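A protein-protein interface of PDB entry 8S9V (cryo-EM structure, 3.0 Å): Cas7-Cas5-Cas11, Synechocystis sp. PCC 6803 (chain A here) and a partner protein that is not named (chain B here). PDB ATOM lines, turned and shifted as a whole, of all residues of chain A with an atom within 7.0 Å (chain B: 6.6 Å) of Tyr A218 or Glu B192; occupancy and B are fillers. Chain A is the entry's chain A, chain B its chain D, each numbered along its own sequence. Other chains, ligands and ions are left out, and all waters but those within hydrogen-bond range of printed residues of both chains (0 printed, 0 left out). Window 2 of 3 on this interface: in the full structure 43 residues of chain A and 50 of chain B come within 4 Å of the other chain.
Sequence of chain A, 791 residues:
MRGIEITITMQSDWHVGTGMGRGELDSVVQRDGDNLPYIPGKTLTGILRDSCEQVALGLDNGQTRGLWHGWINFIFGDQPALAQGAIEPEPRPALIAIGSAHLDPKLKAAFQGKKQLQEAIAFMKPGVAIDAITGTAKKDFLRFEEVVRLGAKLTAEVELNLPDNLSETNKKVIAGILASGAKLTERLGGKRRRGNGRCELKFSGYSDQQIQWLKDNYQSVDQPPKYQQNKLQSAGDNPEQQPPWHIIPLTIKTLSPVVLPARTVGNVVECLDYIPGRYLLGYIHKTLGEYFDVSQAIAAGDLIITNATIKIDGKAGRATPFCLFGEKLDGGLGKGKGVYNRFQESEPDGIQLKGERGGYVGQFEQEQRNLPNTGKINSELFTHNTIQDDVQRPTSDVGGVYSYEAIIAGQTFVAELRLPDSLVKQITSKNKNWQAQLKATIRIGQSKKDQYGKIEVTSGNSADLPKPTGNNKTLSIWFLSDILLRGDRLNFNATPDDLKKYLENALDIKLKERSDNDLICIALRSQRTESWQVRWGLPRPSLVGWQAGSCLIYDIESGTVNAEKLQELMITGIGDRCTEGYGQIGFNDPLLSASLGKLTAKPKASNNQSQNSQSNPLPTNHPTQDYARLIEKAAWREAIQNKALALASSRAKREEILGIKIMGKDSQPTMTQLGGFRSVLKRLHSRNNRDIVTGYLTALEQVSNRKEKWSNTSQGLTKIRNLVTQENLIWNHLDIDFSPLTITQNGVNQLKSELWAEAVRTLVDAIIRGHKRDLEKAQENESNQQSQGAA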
ATOM      1  N   GLY A  58       8.834  -6.219  28.968  1.00  0.00           N
ATOM      2  CA  GLY A  58       9.637  -5.462  29.914  1.00  0.00           C
ATOM      3  C   GLY A  58       9.485  -3.961  29.801  1.00  0.00           C
ATOM      4  O   GLY A  58       9.350  -3.268  30.803  1.00  0.00           O
ATOM      5  N   LEU A  59       9.480  -3.439  28.585  1.00  0.00           N
ATOM      6  CA  LEU A  59       9.328  -2.005  28.386  1.00  0.00           C
ATOM      7  C   LEU A  59       7.962  -1.499  28.820  1.00  0.00           C
ATOM      8  O   LEU A  59       7.845  -0.351  29.251  1.00  0.00           O
ATOM      9  CB  LEU A  59       9.550  -1.666  26.917  1.00  0.00           C
ATOM     10  CG  LEU A  59      10.896  -1.980  26.281  1.00  0.00           C
ATOM     11  CD1 LEU A  59      10.818  -1.675  24.823  1.00  0.00           C
ATOM     12  CD2 LEU A  59      11.990  -1.185  26.901  1.00  0.00           C
ATOM     13  N   ASN A  61       6.634  -2.329  31.437  1.00  0.00           N
ATOM     14  CA  ASN A  61       6.590  -2.573  32.873  1.00  0.00           C
ATOM     15  C   ASN A  61       5.648  -3.724  33.198  1.00  0.00           C
ATOM     16  O   ASN A  61       4.871  -3.669  34.147  1.00  0.00           O
ATOM     17  CB  ASN A  61       6.186  -1.320  33.637  1.00  0.00           C
ATOM     18  CG  ASN A  61       7.266  -0.280  33.646  1.00  0.00           C
ATOM     19  OD1 ASN A  61       7.473   0.416  32.668  1.00  0.00           O
ATOM     20  ND2 ASN A  61       7.976  -0.178  34.752  1.00  0.00           N
ATOM     21  N   LEU A  67       1.702   0.219  24.912  1.00  0.00           N
ATOM     22  CA  LEU A  67       2.324   0.854  23.764  1.00  0.00           C
ATOM     23  C   LEU A  67       3.287  -0.078  23.054  1.00  0.00           C
ATOM     24  O   LEU A  67       3.288  -0.154  21.825  1.00  0.00           O
ATOM     25  CB  LEU A  67       3.051   2.103  24.230  1.00  0.00           C
ATOM     26  CG  LEU A  67       3.717   2.974  23.199  1.00  0.00           C
ATOM     27  CD1 LEU A  67       3.541   4.386  23.622  1.00  0.00           C
ATOM     28  CD2 LEU A  67       5.151   2.626  23.191  1.00  0.00           C
ATOM     29  N   TRP A  68       4.119  -0.789  23.806  1.00  0.00           N
ATOM     30  CA  TRP A  68       5.131  -1.638  23.194  1.00  0.00           C
ATOM     31  C   TRP A  68       4.599  -2.952  22.655  1.00  0.00           C
ATOM     32  O   TRP A  68       5.144  -3.458  21.678  1.00  0.00           O
ATOM     33  CB  TRP A  68       6.278  -1.846  24.170  1.00  0.00           C
ATOM     34  CG  TRP A  68       6.987  -0.561  24.356  1.00  0.00           C
ATOM     35  CD1 TRP A  68       6.799   0.337  25.345  1.00  0.00           C
ATOM     36  CD2 TRP A  68       7.928   0.025  23.459  1.00  0.00           C
ATOM     37  NE1 TRP A  68       7.594   1.429  25.150  1.00  0.00           N
ATOM     38  CE2 TRP A  68       8.296   1.258  23.991  1.00  0.00           C
ATOM     39  CE3 TRP A  68       8.505  -0.385  22.260  1.00  0.00           C
ATOM     40  CZ2 TRP A  68       9.216   2.081  23.374  1.00  0.00           C
ATOM     41  CZ3 TRP A  68       9.410   0.427  21.655  1.00  0.00           C
ATOM     42  CH2 TRP A  68       9.759   1.646  22.207  1.00  0.00           C
ATOM     43  N   VAL A 173      13.211   2.543  15.856  1.00  0.00           N
ATOM     44  CA  VAL A 173      12.510   1.714  16.838  1.00  0.00           C
ATOM     45  C   VAL A 173      12.368   0.281  16.359  1.00  0.00           C
ATOM     46  O   VAL A 173      12.561  -0.662  17.128  1.00  0.00           O
ATOM     47  CB  VAL A 173      11.141   2.296  17.185  1.00  0.00           C
ATOM     48  CG1 VAL A 173      10.486   1.358  18.116  1.00  0.00           C
ATOM     49  CG2 VAL A 173      11.284   3.643  17.812  1.00  0.00           C
ATOM     50  N   TRP A 213      20.622   2.598  20.983  1.00  0.00           N
ATOM     51  CA  TRP A 213      19.710   3.681  20.647  1.00  0.00           C
ATOM     52  C   TRP A 213      18.373   3.526  21.343  1.00  0.00           C
ATOM     53  O   TRP A 213      17.837   4.494  21.887  1.00  0.00           O
ATOM     54  CB  TRP A 213      19.474   3.739  19.151  1.00  0.00           C
ATOM     55  CG  TRP A 213      18.622   4.873  18.767  1.00  0.00           C
ATOM     56  CD1 TRP A 213      19.039   6.088  18.360  1.00  0.00           C
ATOM     57  CD2 TRP A 213      17.197   4.932  18.809  1.00  0.00           C
ATOM     58  NE1 TRP A 213      17.968   6.899  18.108  1.00  0.00           N
ATOM     59  CE2 TRP A 213      16.821   6.211  18.384  1.00  0.00           C
ATOM     60  CE3 TRP A 213      16.200   4.024  19.157  1.00  0.00           C
ATOM     61  CZ2 TRP A 213      15.504   6.606  18.296  1.00  0.00           C
ATOM     62  CZ3 TRP A 213      14.893   4.422  19.067  1.00  0.00           C
ATOM     63  CH2 TRP A 213      14.557   5.700  18.639  1.00  0.00           C
ATOM     64  N   LEU A 214      17.826   2.313  21.362  1.00  0.00           N
ATOM     65  CA  LEU A 214      16.551   2.089  22.037  1.00  0.00           C
ATOM     66  C   LEU A 214      16.650   2.342  23.536  1.00  0.00           C
ATOM     67  O   LEU A 214      15.785   2.999  24.117  1.00  0.00           O
ATOM     68  CB  LEU A 214      16.043   0.680  21.756  1.00  0.00           C
ATOM     69  CG  LEU A 214      14.576   0.487  22.100  1.00  0.00           C
ATOM     70  CD1 LEU A 214      13.789   1.266  21.131  1.00  0.00           C
ATOM     71  CD2 LEU A 214      14.201  -0.941  21.995  1.00  0.00           C
ATOM     72  N   LYS A 215      17.708   1.861  24.174  1.00  0.00           N
ATOM     73  CA  LYS A 215      17.908   2.168  25.581  1.00  0.00           C
ATOM     74  C   LYS A 215      17.916   3.661  25.831  1.00  0.00           C
ATOM     75  O   LYS A 215      17.338   4.140  26.811  1.00  0.00           O
ATOM     76  CB  LYS A 215      19.224   1.568  26.051  1.00  0.00           C
ATOM     77  CG  LYS A 215      19.500   1.720  27.511  1.00  0.00           C
ATOM     78  CD  LYS A 215      20.820   1.086  27.811  1.00  0.00           C
ATOM     79  CE  LYS A 215      21.116   1.066  29.286  1.00  0.00           C
ATOM     80  NZ  LYS A 215      21.352   2.428  29.796  1.00  0.00           N
ATOM     81  N   ASP A 216      18.576   4.411  24.963  1.00  0.00           N
ATOM     82  CA  ASP A 216      18.671   5.849  25.117  1.00  0.00           C
ATOM     83  C   ASP A 216      17.364   6.562  24.831  1.00  0.00           C
ATOM     84  O   ASP A 216      17.205   7.708  25.248  1.00  0.00           O
ATOM     85  CB  ASP A 216      19.764   6.378  24.199  1.00  0.00           C
ATOM     86  CG  ASP A 216      21.126   5.845  24.558  1.00  0.00           C
ATOM     87  OD1 ASP A 216      21.259   5.249  25.640  1.00  0.00           O
ATOM     88  OD2 ASP A 216      22.065   5.995  23.754  1.00  0.00           O
ATOM     89  N   ASN A 217      16.427   5.931  24.136  1.00  0.00           N
ATOM     90  CA  ASN A 217      15.290   6.663  23.612  1.00  0.00           C
ATOM     91  C   ASN A 217      13.913   6.056  23.837  1.00  0.00           C
ATOM     92  O   ASN A 217      12.932   6.645  23.382  1.00  0.00           O
ATOM     93  CB  ASN A 217      15.504   6.914  22.130  1.00  0.00           C
ATOM     94  CG  ASN A 217      16.690   7.791  21.888  1.00  0.00           C
ATOM     95  OD1 ASN A 217      16.591   9.010  21.942  1.00  0.00           O
ATOM     96  ND2 ASN A 217      17.839   7.181  21.679  1.00  0.00           N
ATOM     97  N   TYR A 218      13.805   4.871  24.435  1.00  0.00           N
ATOM     98  CA  TYR A 218      12.502   4.220  24.521  1.00  0.00           C
ATOM     99  C   TYR A 218      11.455   5.091  25.206  1.00  0.00           C
ATOM    100  O   TYR A 218      10.274   5.015  24.865  1.00  0.00           O
ATOM    101  CB  TYR A 218      12.603   2.881  25.230  1.00  0.00           C
ATOM    102  CG  TYR A 218      12.806   2.964  26.701  1.00  0.00           C
ATOM    103  CD1 TYR A 218      14.066   3.132  27.235  1.00  0.00           C
ATOM    104  CD2 TYR A 218      11.741   2.864  27.565  1.00  0.00           C
ATOM    105  CE1 TYR A 218      14.264   3.181  28.584  1.00  0.00           C
ATOM    106  CE2 TYR A 218      11.928   2.931  28.916  1.00  0.00           C
ATOM    107  CZ  TYR A 218      13.193   3.086  29.419  1.00  0.00           C
ATOM    108  OH  TYR A 218      13.386   3.178  30.766  1.00  0.00           O
ATOM    109  N   GLN A 219      11.852   5.919  26.164  1.00  0.00           N
ATOM    110  CA  GLN A 219      10.883   6.768  26.849  1.00  0.00           C
ATOM    111  C   GLN A 219      10.208   7.770  25.930  1.00  0.00           C
ATOM    112  O   GLN A 219       9.165   8.311  26.292  1.00  0.00           O
ATOM    113  CB  GLN A 219      11.567   7.515  27.984  1.00  0.00           C
ATOM    114  CG  GLN A 219      12.149   6.619  29.044  1.00  0.00           C
ATOM    115  CD  GLN A 219      12.670   7.392  30.228  1.00  0.00           C
ATOM    116  OE1 GLN A 219      12.652   8.618  30.236  1.00  0.00           O
ATOM    117  NE2 GLN A 219      13.162   6.679  31.230  1.00  0.00           N
ATOM    118  N   SER A 220      10.776   8.037  24.769  1.00  0.00           N
ATOM    119  CA  SER A 220      10.257   9.012  23.820  1.00  0.00           C
ATOM    120  C   SER A 220       9.280   8.445  22.800  1.00  0.00           C
ATOM    121  O   SER A 220       8.718   9.217  22.022  1.00  0.00           O
ATOM    122  CB  SER A 220      11.410   9.677  23.080  1.00  0.00           C
ATOM    123  OG  SER A 220      11.970   8.782  22.147  1.00  0.00           O
ATOM    124  N   VAL A 221       9.087   7.133  22.762  1.00  0.00           N
ATOM    125  CA  VAL A 221       8.456   6.462  21.630  1.00  0.00           C
ATOM    126  C   VAL A 221       6.941   6.592  21.681  1.00  0.00           C
ATOM    127  O   VAL A 221       6.325   6.520  22.745  1.00  0.00           O
ATOM    128  CB  VAL A 221       8.870   4.985  21.627  1.00  0.00           C
ATOM    129  CG1 VAL A 221       8.180   4.272  20.526  1.00  0.00           C
ATOM    130  CG2 VAL A 221      10.362   4.860  21.485  1.00  0.00           C
ATOM    131  N   ASP A 222       6.340   6.781  20.507  1.00  0.00           N
ATOM    132  CA  ASP A 222       4.904   6.919  20.313  1.00  0.00           C
ATOM    133  C   ASP A 222       4.231   5.592  19.962  1.00  0.00           C
ATOM    134  O   ASP A 222       4.859   4.537  19.873  1.00  0.00           O
ATOM    135  CB  ASP A 222       4.593   7.942  19.226  1.00  0.00           C
ATOM    136  CG  ASP A 222       5.067   9.324  19.576  1.00  0.00           C
ATOM    137  OD1 ASP A 222       5.235   9.604  20.778  1.00  0.00           O
ATOM    138  OD2 ASP A 222       5.255  10.135  18.647  1.00  0.00           O
ATOM    139  N   ALA B 187      16.100  -8.171  36.217  1.00  0.00           N
ATOM    140  CA  ALA B 187      14.714  -7.794  36.504  1.00  0.00           C
ATOM    141  C   ALA B 187      13.933  -7.581  35.209  1.00  0.00           C
ATOM    142  O   ALA B 187      13.511  -6.478  34.876  1.00  0.00           O
ATOM    143  CB  ALA B 187      14.664  -6.551  37.372  1.00  0.00           C
ATOM    144  N   LYS B 190      11.193  -4.904  33.895  1.00  0.00           N
ATOM    145  CA  LYS B 190      11.304  -3.455  33.849  1.00  0.00           C
ATOM    146  C   LYS B 190      12.317  -3.017  32.810  1.00  0.00           C
ATOM    147  O   LYS B 190      13.265  -3.749  32.515  1.00  0.00           O
ATOM    148  CB  LYS B 190      11.702  -2.894  35.212  1.00  0.00           C
ATOM    149  CG  LYS B 190      10.697  -3.209  36.273  1.00  0.00           C
ATOM    150  CD  LYS B 190      11.024  -2.511  37.553  1.00  0.00           C
ATOM    151  CE  LYS B 190      10.020  -2.867  38.608  1.00  0.00           C
ATOM    152  NZ  LYS B 190      10.254  -2.083  39.844  1.00  0.00           N
ATOM    153  N   PRO B 191      12.163  -1.809  32.267  1.00  0.00           N
ATOM    154  CA  PRO B 191      13.086  -1.355  31.223  1.00  0.00           C
ATOM    155  C   PRO B 191      14.527  -1.386  31.655  1.00  0.00           C
ATOM    156  O   PRO B 191      15.402  -1.767  30.875  1.00  0.00           O
ATOM    157  CB  PRO B 191      12.612   0.070  30.951  1.00  0.00           C
ATOM    158  CG  PRO B 191      11.220   0.067  31.322  1.00  0.00           C
ATOM    159  CD  PRO B 191      11.094  -0.835  32.495  1.00  0.00           C
ATOM    160  N   GLU B 192      14.812  -0.953  32.873  1.00  0.00           N
ATOM    161  CA  GLU B 192      16.181  -0.977  33.356  1.00  0.00           C
ATOM    162  C   GLU B 192      16.702  -2.399  33.431  1.00  0.00           C
ATOM    163  O   GLU B 192      17.901  -2.633  33.283  1.00  0.00           O
ATOM    164  CB  GLU B 192      16.250  -0.307  34.723  1.00  0.00           C
ATOM    165  CG  GLU B 192      15.873   1.161  34.679  1.00  0.00           C
ATOM    166  CD  GLU B 192      14.377   1.372  34.535  1.00  0.00           C
ATOM    167  OE1 GLU B 192      13.620   0.421  34.801  1.00  0.00           O
ATOM    168  OE2 GLU B 192      13.957   2.474  34.129  1.00  0.00           O
ATOM    169  N   GLY B 193      15.816  -3.347  33.716  1.00  0.00           N
ATOM    170  CA  GLY B 193      16.188  -4.745  33.762  1.00  0.00           C
ATOM    171  C   GLY B 193      16.247  -5.454  32.432  1.00  0.00           C
ATOM    172  O   GLY B 193      17.059  -6.361  32.258  1.00  0.00           O
ATOM    173  N   ILE B 194      15.382  -5.089  31.492  1.00  0.00           N
ATOM    174  CA  ILE B 194      15.402  -5.739  30.186  1.00  0.00           C
ATOM    175  C   ILE B 194      16.625  -5.332  29.372  1.00  0.00           C
ATOM    176  O   ILE B 194      17.206  -6.154  28.663  1.00  0.00           O
ATOM    177  CB  ILE B 194      14.103  -5.443  29.422  1.00  0.00           C
ATOM    178  CG1 ILE B 194      13.837  -6.537  28.420  1.00  0.00           C
ATOM    179  CG2 ILE B 194      14.247  -4.210  28.618  1.00  0.00           C
ATOM    180  CD1 ILE B 194      13.665  -7.871  29.047  1.00  0.00           C
ATOM    181  N   PHE B 195      17.034  -4.069  29.443  1.00  0.00           N
ATOM    182  CA  PHE B 195      18.295  -3.671  28.826  1.00  0.00           C
ATOM    183  C   PHE B 195      19.511  -4.261  29.515  1.00  0.00           C
ATOM    184  O   PHE B 195      20.518  -4.521  28.859  1.00  0.00           O
ATOM    185  CB  PHE B 195      18.389  -2.161  28.783  1.00  0.00           C
ATOM    186  CG  PHE B 195      17.440  -1.557  27.842  1.00  0.00           C
ATOM    187  CD1 PHE B 195      17.501  -1.859  26.510  1.00  0.00           C
ATOM    188  CD2 PHE B 195      16.458  -0.725  28.282  1.00  0.00           C
ATOM    189  CE1 PHE B 195      16.618  -1.325  25.639  1.00  0.00           C
ATOM    190  CE2 PHE B 195      15.570  -0.186  27.408  1.00  0.00           C
ATOM    191  CZ  PHE B 195      15.648  -0.489  26.090  1.00  0.00           C
ATOM    192  N   SER B 196      19.454  -4.475  30.819  1.00  0.00           N
ATOM    193  CA  SER B 196      20.543  -5.168  31.489  1.00  0.00           C
ATOM    194  C   SER B 196      20.771  -6.552  30.916  1.00  0.00           C
ATOM    195  O   SER B 196      21.913  -6.983  30.757  1.00  0.00           O
ATOM    196  CB  SER B 196      20.239  -5.282  32.971  1.00  0.00           C
ATOM    197  OG  SER B 196      21.262  -5.987  33.629  1.00  0.00           O
ATOM    198  N   ALA B 197      19.700  -7.261  30.592  1.00  0.00           N
ATOM    199  CA  ALA B 197      19.829  -8.557  29.945  1.00  0.00           C
ATOM    200  C   ALA B 197      20.519  -8.459  28.595  1.00  0.00           C
ATOM    201  O   ALA B 197      21.271  -9.357  28.210  1.00  0.00           O
ATOM    202  CB  ALA B 197      18.446  -9.181  29.790  1.00  0.00           C
ATOM    203  N   ASP B 200      24.175  -5.108  29.967  1.00  0.00           N
ATOM    204  CA  ASP B 200      24.947  -4.890  31.191  1.00  0.00           C
ATOM    205  C   ASP B 200      25.369  -6.153  31.922  1.00  0.00           C
ATOM    206  O   ASP B 200      26.100  -6.049  32.908  1.00  0.00           O
ATOM    207  CB  ASP B 200      24.163  -4.014  32.169  1.00  0.00           C
ATOM    208  CG  ASP B 200      23.713  -2.706  31.554  1.00  0.00           C
ATOM    209  OD1 ASP B 200      24.496  -2.121  30.782  1.00  0.00           O
ATOM    210  OD2 ASP B 200      22.584  -2.260  31.845  1.00  0.00           O
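Printed residues of chain B within 4 Å of Leu A59: Pro B191 and Phe B195.
Of the printed residues of chain B, Asn A61 touches Pro B191 (3.8 Å).
Tyr A218 touches just these residues of chain B: Pro B191, Glu B192 and Phe B195.
Gln A219 touches none of the printed residues of chain B.
Of the printed residues of chain A, Pro B191 touches Gly A58 (3.4 Å), Leu A59 (3.98 Å), Asn A61 (3.8 Å) and Tyr A218 (3.2 Å).
Of the printed residues of chain A, Phe B195 touches Leu A59 (3.8 Å), Leu A214 (3.9 Å), Lys A215 (3.5 Å) and Tyr A218 (3.6 Å).
The nearest residue of chain A that does not touch Glu B192 is Gln A219 (5.2 Å).
The nearest printed residue of chain B that does not touch Leu A214 is Ile B194 (7.4 Å).
Of the 10 printed residues of chain B, 4 touch a printed residue of chain A.
Hydrophobic or aromatic side chains of chain B within 4 Å of the printed part of chain A: Pro B191 and Phe B195.
Along chain A the printed residues that touch a printed residue of chain B span positions 58 to 218.
Among the printed residues, 10 pairs touch across the chains.
Among the printed residues, no Asp or Glu carboxylate lies within 4 Å of a Lys or Arg side-chain nitrogen of the other chain.
The backbone carbonyl oxygen of Gly A58 sits close to the backbone nitrogen of Pro B191.
The side-chain hydroxyl (OH) of Tyr A218 lies within hydrogen-bond range of the side-chain carboxylate (OE2) of Glu B192 (3.5 Å).
Among the printed residues, pairs that only touch across the chains: Tyr A218 with Pro B191, Lys A215 with Phe B195, Gly A58 with Lys B190, Tyr A218 with Phe B195, Leu A59 with Phe B195, Asn A61 with Pro B191, Leu A214 with Phe B195 and Leu A59 with Pro B191.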
